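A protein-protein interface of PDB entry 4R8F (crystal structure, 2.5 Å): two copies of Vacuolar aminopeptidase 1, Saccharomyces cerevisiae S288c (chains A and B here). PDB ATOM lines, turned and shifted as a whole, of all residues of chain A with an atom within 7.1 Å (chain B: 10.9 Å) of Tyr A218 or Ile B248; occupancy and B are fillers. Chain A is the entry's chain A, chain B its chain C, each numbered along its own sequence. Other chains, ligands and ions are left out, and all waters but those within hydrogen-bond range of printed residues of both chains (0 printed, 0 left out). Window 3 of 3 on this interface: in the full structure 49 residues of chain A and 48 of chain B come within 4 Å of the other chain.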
ATOM      1  N   ILE A 131      17.382  20.049   2.835  1.00  0.00           N
ATOM      2  CA  ILE A 131      18.433  20.842   2.225  1.00  0.00           C
ATOM      3  C   ILE A 131      19.301  21.347   3.361  1.00  0.00           C
ATOM      4  O   ILE A 131      18.799  21.629   4.445  1.00  0.00           O
ATOM      5  CB  ILE A 131      17.862  21.993   1.363  1.00  0.00           C
ATOM      6  CG1 ILE A 131      18.971  22.640   0.527  1.00  0.00           C
ATOM      7  CG2 ILE A 131      17.154  23.036   2.218  1.00  0.00           C
ATOM      8  CD1 ILE A 131      18.457  23.520  -0.591  1.00  0.00           C
ATOM      9  N   LEU A 135      26.762  27.998   3.993  1.00  0.00           N
ATOM     10  CA  LEU A 135      26.585  29.309   3.379  1.00  0.00           C
ATOM     11  C   LEU A 135      27.800  30.157   3.696  1.00  0.00           C
ATOM     12  O   LEU A 135      28.329  30.092   4.800  1.00  0.00           O
ATOM     13  CB  LEU A 135      25.358  30.025   3.943  1.00  0.00           C
ATOM     14  CG  LEU A 135      24.015  29.303   3.939  1.00  0.00           C
ATOM     15  CD1 LEU A 135      22.938  30.254   4.432  1.00  0.00           C
ATOM     16  CD2 LEU A 135      23.667  28.790   2.555  1.00  0.00           C
ATOM     17  N   VAL A 150      23.657  25.273   7.816  1.00  0.00           N
ATOM     18  CA  VAL A 150      22.233  25.403   7.584  1.00  0.00           C
ATOM     19  C   VAL A 150      21.662  24.000   7.365  1.00  0.00           C
ATOM     20  O   VAL A 150      22.321  23.140   6.789  1.00  0.00           O
ATOM     21  CB  VAL A 150      22.013  26.381   6.397  1.00  0.00           C
ATOM     22  CG1 VAL A 150      21.125  25.805   5.305  1.00  0.00           C
ATOM     23  CG2 VAL A 150      21.506  27.724   6.902  1.00  0.00           C
ATOM     24  N   ASP A 151      20.449  23.768   7.853  1.00  0.00           N
ATOM     25  CA  ASP A 151      19.851  22.432   7.859  1.00  0.00           C
ATOM     26  C   ASP A 151      18.338  22.570   8.025  1.00  0.00           C
ATOM     27  O   ASP A 151      17.870  23.221   8.960  1.00  0.00           O
ATOM     28  CB  ASP A 151      20.451  21.611   9.008  1.00  0.00           C
ATOM     29  CG  ASP A 151      19.990  20.150   9.021  1.00  0.00           C
ATOM     30  OD1 ASP A 151      19.317  19.701   8.071  1.00  0.00           O
ATOM     31  OD2 ASP A 151      20.314  19.441  10.002  1.00  0.00           O
ATOM     32  N   SER A 152      17.580  21.966   7.111  1.00  0.00           N
ATOM     33  CA  SER A 152      16.118  22.076   7.128  1.00  0.00           C
ATOM     34  C   SER A 152      15.440  20.979   7.948  1.00  0.00           C
ATOM     35  O   SER A 152      14.243  21.061   8.211  1.00  0.00           O
ATOM     36  CB  SER A 152      15.567  22.055   5.701  1.00  0.00           C
ATOM     37  OG  SER A 152      15.633  20.754   5.145  1.00  0.00           O
ATOM     38  N   THR A 153      16.195  19.956   8.342  1.00  0.00           N
ATOM     39  CA  THR A 153      15.647  18.836   9.109  1.00  0.00           C
ATOM     40  C   THR A 153      14.782  19.358  10.264  1.00  0.00           C
ATOM     41  O   THR A 153      15.205  20.272  10.967  1.00  0.00           O
ATOM     42  CB  THR A 153      16.780  17.961   9.678  1.00  0.00           C
ATOM     43  OG1 THR A 153      17.688  17.618   8.625  1.00  0.00           O
ATOM     44  CG2 THR A 153      16.243  16.681  10.309  1.00  0.00           C
ATOM     45  N   LEU A 155      12.233  19.170   8.052  1.00  0.00           N
ATOM     46  CA  LEU A 155      11.421  19.558   6.895  1.00  0.00           C
ATOM     47  C   LEU A 155      12.021  19.038   5.593  1.00  0.00           C
ATOM     48  O   LEU A 155      13.107  19.469   5.208  1.00  0.00           O
ATOM     49  CB  LEU A 155      11.293  21.085   6.804  1.00  0.00           C
ATOM     50  CG  LEU A 155      10.619  21.625   5.533  1.00  0.00           C
ATOM     51  CD1 LEU A 155       9.135  21.294   5.508  1.00  0.00           C
ATOM     52  CD2 LEU A 155      10.833  23.123   5.403  1.00  0.00           C
ATOM     53  N   PRO A 156      11.312  18.124   4.901  1.00  0.00           N
ATOM     54  CA  PRO A 156      11.750  17.776   3.563  1.00  0.00           C
ATOM     55  C   PRO A 156      11.302  18.872   2.625  1.00  0.00           C
ATOM     56  O   PRO A 156      10.103  19.050   2.424  1.00  0.00           O
ATOM     57  CB  PRO A 156      11.004  16.470   3.263  1.00  0.00           C
ATOM     58  CG  PRO A 156      10.183  16.161   4.475  1.00  0.00           C
ATOM     59  CD  PRO A 156      10.058  17.436   5.238  1.00  0.00           C
ATOM     60  N   VAL A 157      12.251  19.619   2.077  1.00  0.00           N
ATOM     61  CA  VAL A 157      11.918  20.733   1.200  1.00  0.00           C
ATOM     62  C   VAL A 157      11.701  20.279  -0.234  1.00  0.00           C
ATOM     63  O   VAL A 157      11.283  21.079  -1.075  1.00  0.00           O
ATOM     64  CB  VAL A 157      12.988  21.848   1.226  1.00  0.00           C
ATOM     65  CG1 VAL A 157      13.095  22.435   2.625  1.00  0.00           C
ATOM     66  CG2 VAL A 157      14.341  21.350   0.737  1.00  0.00           C
ATOM     67  N   CYS A 158      11.990  19.016  -0.531  1.00  0.00           N
ATOM     68  CA  CYS A 158      11.855  18.547  -1.895  1.00  0.00           C
ATOM     69  C   CYS A 158      11.948  17.034  -2.029  1.00  0.00           C
ATOM     70  O   CYS A 158      12.172  16.318  -1.054  1.00  0.00           O
ATOM     71  CB  CYS A 158      12.928  19.203  -2.760  1.00  0.00           C
ATOM     72  SG  CYS A 158      14.498  18.311  -2.779  1.00  0.00           S
ATOM     73  N   PRO A 183      10.510  18.759  -7.636  1.00  0.00           N
ATOM     74  CA  PRO A 183       9.468  19.580  -7.018  1.00  0.00           C
ATOM     75  C   PRO A 183       9.857  20.153  -5.648  1.00  0.00           C
ATOM     76  O   PRO A 183      10.056  19.401  -4.691  1.00  0.00           O
ATOM     77  CB  PRO A 183       8.307  18.595  -6.870  1.00  0.00           C
ATOM     78  CG  PRO A 183       8.455  17.693  -8.042  1.00  0.00           C
ATOM     79  CD  PRO A 183       9.933  17.583  -8.310  1.00  0.00           C
ATOM     80  N   VAL A 184       9.958  21.481  -5.571  1.00  0.00           N
ATOM     81  CA  VAL A 184      10.252  22.180  -4.314  1.00  0.00           C
ATOM     82  C   VAL A 184       9.004  22.234  -3.434  1.00  0.00           C
ATOM     83  O   VAL A 184       8.917  23.040  -2.508  1.00  0.00           O
ATOM     84  CB  VAL A 184      10.786  23.623  -4.539  1.00  0.00           C
ATOM     85  CG1 VAL A 184      12.037  23.617  -5.412  1.00  0.00           C
ATOM     86  CG2 VAL A 184       9.703  24.542  -5.108  1.00  0.00           C
ATOM     87  N   CYS A 212      16.558  30.970  -6.760  1.00  0.00           N
ATOM     88  CA  CYS A 212      15.244  31.595  -6.674  1.00  0.00           C
ATOM     89  C   CYS A 212      15.114  32.291  -5.326  1.00  0.00           C
ATOM     90  O   CYS A 212      15.640  31.810  -4.320  1.00  0.00           O
ATOM     91  CB  CYS A 212      14.114  30.581  -6.911  1.00  0.00           C
ATOM     92  SG  CYS A 212      13.449  29.751  -5.449  1.00  0.00           S
ATOM     93  N   ILE A 213      14.428  33.430  -5.320  1.00  0.00           N
ATOM     94  CA  ILE A 213      14.382  34.294  -4.142  1.00  0.00           C
ATOM     95  C   ILE A 213      13.852  33.572  -2.902  1.00  0.00           C
ATOM     96  O   ILE A 213      14.286  33.857  -1.784  1.00  0.00           O
ATOM     97  CB  ILE A 213      13.547  35.575  -4.399  1.00  0.00           C
ATOM     98  CG1 ILE A 213      13.837  36.639  -3.334  1.00  0.00           C
ATOM     99  CG2 ILE A 213      12.053  35.262  -4.441  1.00  0.00           C
ATOM    100  CD1 ILE A 213      15.305  36.977  -3.174  1.00  0.00           C
ATOM    101  N   HIS A 214      12.929  32.635  -3.101  1.00  0.00           N
ATOM    102  CA  HIS A 214      12.335  31.918  -1.984  1.00  0.00           C
ATOM    103  C   HIS A 214      13.369  31.043  -1.280  1.00  0.00           C
ATOM    104  O   HIS A 214      13.455  31.049  -0.053  1.00  0.00           O
ATOM    105  CB  HIS A 214      11.153  31.064  -2.441  1.00  0.00           C
ATOM    106  CG  HIS A 214      10.149  30.799  -1.360  1.00  0.00           C
ATOM    107  ND1 HIS A 214      10.465  30.842  -0.016  1.00  0.00           N
ATOM    108  CD2 HIS A 214       8.836  30.477  -1.425  1.00  0.00           C
ATOM    109  CE1 HIS A 214       9.389  30.565   0.697  1.00  0.00           C
ATOM    110  NE2 HIS A 214       8.386  30.336  -0.133  1.00  0.00           N
ATOM    111  N   LEU A 215      14.148  30.296  -2.055  1.00  0.00           N
ATOM    112  CA  LEU A 215      15.201  29.458  -1.491  1.00  0.00           C
ATOM    113  C   LEU A 215      16.220  30.298  -0.728  1.00  0.00           C
ATOM    114  O   LEU A 215      16.614  29.950   0.384  1.00  0.00           O
ATOM    115  CB  LEU A 215      15.904  28.666  -2.592  1.00  0.00           C
ATOM    116  CG  LEU A 215      17.029  27.736  -2.135  1.00  0.00           C
ATOM    117  CD1 LEU A 215      16.512  26.694  -1.157  1.00  0.00           C
ATOM    118  CD2 LEU A 215      17.675  27.072  -3.339  1.00  0.00           C
ATOM    119  N   LEU A 216      16.640  31.402  -1.339  1.00  0.00           N
ATOM    120  CA  LEU A 216      17.572  32.332  -0.709  1.00  0.00           C
ATOM    121  C   LEU A 216      17.008  32.914   0.580  1.00  0.00           C
ATOM    122  O   LEU A 216      17.718  33.019   1.581  1.00  0.00           O
ATOM    123  CB  LEU A 216      17.925  33.465  -1.671  1.00  0.00           C
ATOM    124  CG  LEU A 216      18.812  33.062  -2.850  1.00  0.00           C
ATOM    125  CD1 LEU A 216      18.978  34.230  -3.809  1.00  0.00           C
ATOM    126  CD2 LEU A 216      20.169  32.566  -2.365  1.00  0.00           C
ATOM    127  N   ARG A 217      15.733  33.296   0.553  1.00  0.00           N
ATOM    128  CA  ARG A 217      15.066  33.799   1.755  1.00  0.00           C
ATOM    129  C   ARG A 217      15.026  32.727   2.834  1.00  0.00           C
ATOM    130  O   ARG A 217      15.219  33.020   4.013  1.00  0.00           O
ATOM    131  CB  ARG A 217      13.644  34.280   1.444  1.00  0.00           C
ATOM    132  CG  ARG A 217      13.583  35.628   0.744  1.00  0.00           C
ATOM    133  CD  ARG A 217      12.240  36.310   0.955  1.00  0.00           C
ATOM    134  NE  ARG A 217      12.065  37.441   0.041  1.00  0.00           N
ATOM    135  CZ  ARG A 217      11.154  37.519  -0.934  1.00  0.00           C
ATOM    136  NH1 ARG A 217      10.267  36.547  -1.147  1.00  0.00           N
ATOM    137  NH2 ARG A 217      11.116  38.605  -1.699  1.00  0.00           N
ATOM    138  N   TYR A 218      14.783  31.487   2.416  1.00  0.00           N
ATOM    139  CA  TYR A 218      14.701  30.361   3.337  1.00  0.00           C
ATOM    140  C   TYR A 218      16.040  30.030   4.001  1.00  0.00           C
ATOM    141  O   TYR A 218      16.093  29.852   5.219  1.00  0.00           O
ATOM    142  CB  TYR A 218      14.155  29.121   2.628  1.00  0.00           C
ATOM    143  CG  TYR A 218      14.038  27.934   3.548  1.00  0.00           C
ATOM    144  CD1 TYR A 218      13.094  27.916   4.570  1.00  0.00           C
ATOM    145  CD2 TYR A 218      14.884  26.839   3.413  1.00  0.00           C
ATOM    146  CE1 TYR A 218      12.988  26.836   5.429  1.00  0.00           C
ATOM    147  CE2 TYR A 218      14.787  25.751   4.265  1.00  0.00           C
ATOM    148  CZ  TYR A 218      13.839  25.755   5.272  1.00  0.00           C
ATOM    149  OH  TYR A 218      13.744  24.677   6.122  1.00  0.00           O
ATOM    150  N   VAL A 219      17.114  29.943   3.217  1.00  0.00           N
ATOM    151  CA  VAL A 219      18.432  29.637   3.791  1.00  0.00           C
ATOM    152  C   VAL A 219      18.947  30.802   4.633  1.00  0.00           C
ATOM    153  O   VAL A 219      19.579  30.586   5.664  1.00  0.00           O
ATOM    154  CB  VAL A 219      19.500  29.235   2.738  1.00  0.00           C
ATOM    155  CG1 VAL A 219      19.028  28.040   1.925  1.00  0.00           C
ATOM    156  CG2 VAL A 219      19.880  30.401   1.837  1.00  0.00           C
ATOM    157  N   ALA A 220      18.665  32.028   4.192  1.00  0.00           N
ATOM    158  CA  ALA A 220      19.020  33.232   4.954  1.00  0.00           C
ATOM    159  C   ALA A 220      18.381  33.227   6.340  1.00  0.00           C
ATOM    160  O   ALA A 220      19.012  33.623   7.323  1.00  0.00           O
ATOM    161  CB  ALA A 220      18.608  34.486   4.196  1.00  0.00           C
ATOM    162  N   LYS A 221      17.132  32.771   6.405  1.00  0.00           N
ATOM    163  CA  LYS A 221      16.399  32.679   7.665  1.00  0.00           C
ATOM    164  C   LYS A 221      17.048  31.673   8.624  1.00  0.00           C
ATOM    165  O   LYS A 221      17.232  31.963   9.808  1.00  0.00           O
ATOM    166  CB  LYS A 221      14.942  32.281   7.409  1.00  0.00           C
ATOM    167  CG  LYS A 221      14.007  32.621   8.564  1.00  0.00           C
ATOM    168  CD  LYS A 221      13.048  31.482   8.902  1.00  0.00           C
ATOM    169  CE  LYS A 221      11.720  31.600   8.165  1.00  0.00           C
ATOM    170  NZ  LYS A 221      10.813  32.594   8.810  1.00  0.00           N
ATOM    171  N   LEU A 222      17.396  30.499   8.103  1.00  0.00           N
ATOM    172  CA  LEU A 222      18.043  29.450   8.895  1.00  0.00           C
ATOM    173  C   LEU A 222      19.382  29.909   9.473  1.00  0.00           C
ATOM    174  O   LEU A 222      19.697  29.617  10.624  1.00  0.00           O
ATOM    175  CB  LEU A 222      18.277  28.202   8.040  1.00  0.00           C
ATOM    176  CG  LEU A 222      17.083  27.434   7.473  1.00  0.00           C
ATOM    177  CD1 LEU A 222      17.575  26.401   6.472  1.00  0.00           C
ATOM    178  CD2 LEU A 222      16.270  26.770   8.573  1.00  0.00           C
ATOM    179  N   ALA A 223      20.169  30.619   8.668  1.00  0.00           N
ATOM    180  CA  ALA A 223      21.486  31.100   9.094  1.00  0.00           C
ATOM    181  C   ALA A 223      21.413  32.300  10.043  1.00  0.00           C
ATOM    182  O   ALA A 223      22.344  32.545  10.807  1.00  0.00           O
ATOM    183  CB  ALA A 223      22.330  31.451   7.881  1.00  0.00           C
ATOM    184  N   VAL A 227      19.442  38.162   3.073  1.00  0.00           N
ATOM    185  CA  VAL A 227      19.672  37.644   1.728  1.00  0.00           C
ATOM    186  C   VAL A 227      20.802  38.420   1.053  1.00  0.00           C
ATOM    187  O   VAL A 227      21.652  37.834   0.385  1.00  0.00           O
ATOM    188  CB  VAL A 227      18.400  37.745   0.862  1.00  0.00           C
ATOM    189  CG1 VAL A 227      18.687  37.346  -0.580  1.00  0.00           C
ATOM    190  CG2 VAL A 227      17.286  36.882   1.440  1.00  0.00           C
ATOM    191  N   THR B 244       4.774  13.035   5.993  1.00  0.00           N
ATOM    192  CA  THR B 244       5.098  14.403   6.365  1.00  0.00           C
ATOM    193  C   THR B 244       4.488  15.399   5.406  1.00  0.00           C
ATOM    194  O   THR B 244       4.333  15.124   4.215  1.00  0.00           O
ATOM    195  CB  THR B 244       6.620  14.675   6.349  1.00  0.00           C
ATOM    196  OG1 THR B 244       7.279  13.727   5.497  1.00  0.00           O
ATOM    197  CG2 THR B 244       7.197  14.594   7.740  1.00  0.00           C
ATOM    198  N   ILE B 245       4.162  16.567   5.948  1.00  0.00           N
ATOM    199  CA  ILE B 245       3.987  17.760   5.150  1.00  0.00           C
ATOM    200  C   ILE B 245       5.388  18.143   4.693  1.00  0.00           C
ATOM    201  O   ILE B 245       6.334  18.081   5.478  1.00  0.00           O
ATOM    202  CB  ILE B 245       3.377  18.912   5.972  1.00  0.00           C
ATOM    203  CG1 ILE B 245       1.942  18.572   6.386  1.00  0.00           C
ATOM    204  CG2 ILE B 245       3.415  20.215   5.183  1.00  0.00           C
ATOM    205  CD1 ILE B 245       0.935  18.632   5.256  1.00  0.00           C
ATOM    206  N   GLY B 246       5.523  18.532   3.431  1.00  0.00           N
ATOM    207  CA  GLY B 246       6.832  18.800   2.858  1.00  0.00           C
ATOM    208  C   GLY B 246       6.823  19.896   1.819  1.00  0.00           C
ATOM    209  O   GLY B 246       5.784  20.493   1.527  1.00  0.00           O
ATOM    210  N   GLY B 247       7.995  20.143   1.244  1.00  0.00           N
ATOM    211  CA  GLY B 247       8.182  21.242   0.312  1.00  0.00           C
ATOM    212  C   GLY B 247       8.530  22.505   1.067  1.00  0.00           C
ATOM    213  O   GLY B 247       8.193  22.657   2.240  1.00  0.00           O
ATOM    214  N   ILE B 248       9.192  23.426   0.381  1.00  0.00           N
ATOM    215  CA  ILE B 248       9.683  24.648   1.007  1.00  0.00           C
ATOM    216  C   ILE B 248       8.568  25.546   1.553  1.00  0.00           C
ATOM    217  O   ILE B 248       8.754  26.204   2.577  1.00  0.00           O
ATOM    218  CB  ILE B 248      10.593  25.434   0.033  1.00  0.00           C
ATOM    219  CG1 ILE B 248      11.520  26.377   0.805  1.00  0.00           C
ATOM    220  CG2 ILE B 248       9.770  26.171  -1.027  1.00  0.00           C
ATOM    221  CD1 ILE B 248      12.976  26.203   0.428  1.00  0.00           C
ATOM    222  N   GLY B 249       7.420  25.565   0.877  1.00  0.00           N
ATOM    223  CA  GLY B 249       6.244  26.301   1.351  1.00  0.00           C
ATOM    224  C   GLY B 249       5.184  25.416   1.996  1.00  0.00           C
ATOM    225  O   GLY B 249       4.061  25.861   2.220  1.00  0.00           O
ATOM    226  N   LYS B 250       5.541  24.169   2.299  1.00  0.00           N
ATOM    227  CA  LYS B 250       4.618  23.179   2.874  1.00  0.00           C
ATOM    228  C   LYS B 250       3.400  22.894   1.991  1.00  0.00           C
ATOM    229  O   LYS B 250       2.304  22.641   2.488  1.00  0.00           O
ATOM    230  CB  LYS B 250       4.189  23.593   4.283  1.00  0.00           C
ATOM    231  CG  LYS B 250       5.355  23.770   5.236  1.00  0.00           C
ATOM    232  CD  LYS B 250       4.989  23.357   6.651  1.00  0.00           C
ATOM    233  CE  LYS B 250       6.155  23.572   7.602  1.00  0.00           C
ATOM    234  NZ  LYS B 250       5.833  23.119   8.983  1.00  0.00           N
ATOM    235  N   HIS B 251       3.613  22.905   0.678  1.00  0.00           N
ATOM    236  CA  HIS B 251       2.545  22.683  -0.289  1.00  0.00           C
ATOM    237  C   HIS B 251       2.285  21.204  -0.562  1.00  0.00           C
ATOM    238  O   HIS B 251       1.282  20.856  -1.188  1.00  0.00           O
ATOM    239  CB  HIS B 251       2.871  23.396  -1.606  1.00  0.00           C
ATOM    240  CG  HIS B 251       2.933  24.886  -1.478  1.00  0.00           C
ATOM    241  ND1 HIS B 251       3.836  25.662  -2.175  1.00  0.00           N
ATOM    242  CD2 HIS B 251       2.211  25.743  -0.714  1.00  0.00           C
ATOM    243  CE1 HIS B 251       3.659  26.932  -1.855  1.00  0.00           C
ATOM    244  NE2 HIS B 251       2.682  27.008  -0.969  1.00  0.00           N
ATOM    245  N   PHE B 252       3.176  20.335  -0.093  1.00  0.00           N
ATOM    246  CA  PHE B 252       3.093  18.921  -0.422  1.00  0.00           C
ATOM    247  C   PHE B 252       2.887  18.035   0.786  1.00  0.00           C
ATOM    248  O   PHE B 252       3.137  18.429   1.921  1.00  0.00           O
ATOM    249  CB  PHE B 252       4.349  18.483  -1.170  1.00  0.00           C
ATOM    250  CG  PHE B 252       4.435  19.039  -2.556  1.00  0.00           C
ATOM    251  CD1 PHE B 252       3.608  18.549  -3.556  1.00  0.00           C
ATOM    252  CD2 PHE B 252       5.326  20.057  -2.863  1.00  0.00           C
ATOM    253  CE1 PHE B 252       3.671  19.061  -4.841  1.00  0.00           C
ATOM    254  CE2 PHE B 252       5.396  20.573  -4.147  1.00  0.00           C
ATOM    255  CZ  PHE B 252       4.567  20.074  -5.137  1.00  0.00           C
ATOM    256  N   LEU B 253       2.424  16.827   0.502  1.00  0.00           N
ATOM    257  CA  LEU B 253       2.231  15.801   1.498  1.00  0.00           C
ATOM    258  C   LEU B 253       2.804  14.515   0.932  1.00  0.00           C
ATOM    259  O   LEU B 253       2.385  14.079  -0.135  1.00  0.00           O
ATOM    260  CB  LEU B 253       0.741  15.646   1.780  1.00  0.00           C
ATOM    261  CG  LEU B 253       0.358  14.758   2.962  1.00  0.00           C
ATOM    262  CD1 LEU B 253      -0.890  15.304   3.634  1.00  0.00           C
ATOM    263  CD2 LEU B 253       0.154  13.311   2.535  1.00  0.00           C
ATOM    264  N   PHE B 254       3.774  13.928   1.631  1.00  0.00           N
ATOM    265  CA  PHE B 254       4.359  12.645   1.232  1.00  0.00           C
ATOM    266  C   PHE B 254       3.914  11.568   2.196  1.00  0.00           C
ATOM    267  O   PHE B 254       4.084  11.718   3.405  1.00  0.00           O
ATOM    268  CB  PHE B 254       5.886  12.697   1.265  1.00  0.00           C
ATOM    269  CG  PHE B 254       6.464  13.929   0.652  1.00  0.00           C
ATOM    270  CD1 PHE B 254       6.115  14.306  -0.630  1.00  0.00           C
ATOM    271  CD2 PHE B 254       7.374  14.703   1.349  1.00  0.00           C
ATOM    272  CE1 PHE B 254       6.651  15.445  -1.207  1.00  0.00           C
ATOM    273  CE2 PHE B 254       7.918  15.841   0.780  1.00  0.00           C
ATOM    274  CZ  PHE B 254       7.557  16.214  -0.500  1.00  0.00           C
ATOM    275  N   ASN B 363      -3.332  21.053  -4.896  1.00  0.00           N
ATOM    276  CA  ASN B 363      -4.005  22.063  -4.074  1.00  0.00           C
ATOM    277  C   ASN B 363      -5.035  22.934  -4.802  1.00  0.00           C
ATOM    278  O   ASN B 363      -5.254  24.084  -4.418  1.00  0.00           O
ATOM    279  CB  ASN B 363      -2.968  22.956  -3.378  1.00  0.00           C
ATOM    280  CG  ASN B 363      -2.001  22.166  -2.510  1.00  0.00           C
ATOM    281  OD1 ASN B 363      -2.413  21.320  -1.714  1.00  0.00           O
ATOM    282  ND2 ASN B 363      -0.709  22.445  -2.650  1.00  0.00           N
ATOM    283  N   SER B 443      -0.791  19.273   0.088  1.00  0.00           N
ATOM    284  CA  SER B 443      -1.070  19.275   1.522  1.00  0.00           C
ATOM    285  C   SER B 443      -2.498  19.744   1.812  1.00  0.00           C
ATOM    286  O   SER B 443      -3.069  19.397   2.845  1.00  0.00           O
ATOM    287  CB  SER B 443      -0.075  20.164   2.260  1.00  0.00           C
ATOM    288  OG  SER B 443      -0.105  21.477   1.737  1.00  0.00           O
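Gly B247 touches Leu A155 (O to CD1, 3.7 Å).
CG of Pro A156 touches OG1 of Thr B244, at 3.9 Å.
Pro A156 touches Ile B245 (CD to O, 3.8 Å).
Pro A156 touches Gly B246.
Gly B247 touches Val A157 (CA to O, 3.4 Å).
O of Val A184 touches CA of Gly B247, 3.4 Å away.
Leu A215 touches Ile B248 (CD1 to CD1, 3.9 Å).
CD1 of Ile B248 touches CD2 of Tyr A218, 3.6 Å away.
Hydrophobic or aromatic side chains of chain A that line the printed part of chain B: Leu A155, Pro A156, Leu A215 and Tyr A218.
Among the printed residues, no Asp or Glu carboxylate lies within 4 Å of a Lys or Arg side-chain nitrogen of the other chain.
O of Pro A156 sits at hydrogen-bond distance from N of Gly B247 (2.7 Å).
The backbone carbonyl oxygen (O) of Val A157 lies within hydrogen-bond range of the backbone NH (N) of Ile B248, at 3.5 Å.
O of Val A184 sits at hydrogen-bond distance from N of Ile B248.
No position is printed for both chains.
The side-chain hydroxyl (OG) of Ser A152 lies within hydrogen-bond range of the backbone carbonyl oxygen (O) of Leu A155 (2.8 Å).
The side-chain sulfur of Cys A212 is in hydrogen-bond range of the backbone NH of Leu A215, at 3.5 Å.
O of Thr B244 sits at hydrogen-bond distance from N of Phe B254, 2.9 Å away.
The backbone carbonyl oxygen (O) of Gly B246 is in hydrogen-bond range of the backbone NH (N) of His B251, at 3.4 Å.
The backbone NH (N) of Gly B246 is in hydrogen-bond range of the backbone carbonyl oxygen (O) of Phe B252 (2.8 Å).
Ile A131 touches none of the printed residues of chain B.
Leu A135 touches none of the printed residues of chain B.
No residue of chain B comes within 4 Å of Ser A152.
Of chain B, only Gly B247 (3.7 Å) comes within 4 Å of Leu A155.
Val A157 touches just these residues of chain B: Gly B247 and Ile B248.
Of chain B, only Ile B248 comes within 4 Å of Leu A215.
Tyr A218 touches one residue of chain B.
Val A219 touches none of the printed residues of chain B.
No residue of chain B comes within 4 Å of Ala A220.
No residue of chain B comes within 4 Å of Lys A221.
Leu A222 touches none of the printed residues of chain B.
Val A227 touches none of the printed residues of chain B.
Of the printed residues of chain A, Thr B244 touches Pro A156.
Printed residues of chain A within 4 Å of Gly B247: Leu A155, Pro A156, Val A157 and Val A184.
Ile B248 touches just these residues of chain A: Val A157 (3.5 Å), Val A184 (2.9 Å), Leu A215 (3.9 Å) and Tyr A218 (3.6 Å).
The nearest residue of chain B that does not touch Tyr A218 is Gly B247 (7.1 Å).
The nearest residue of chain A that does not touch Ile B248 is His A214 (4.4 Å).
The nearest printed residue of chain A that does not touch Ile B245 is Leu A155 (4.3 Å).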
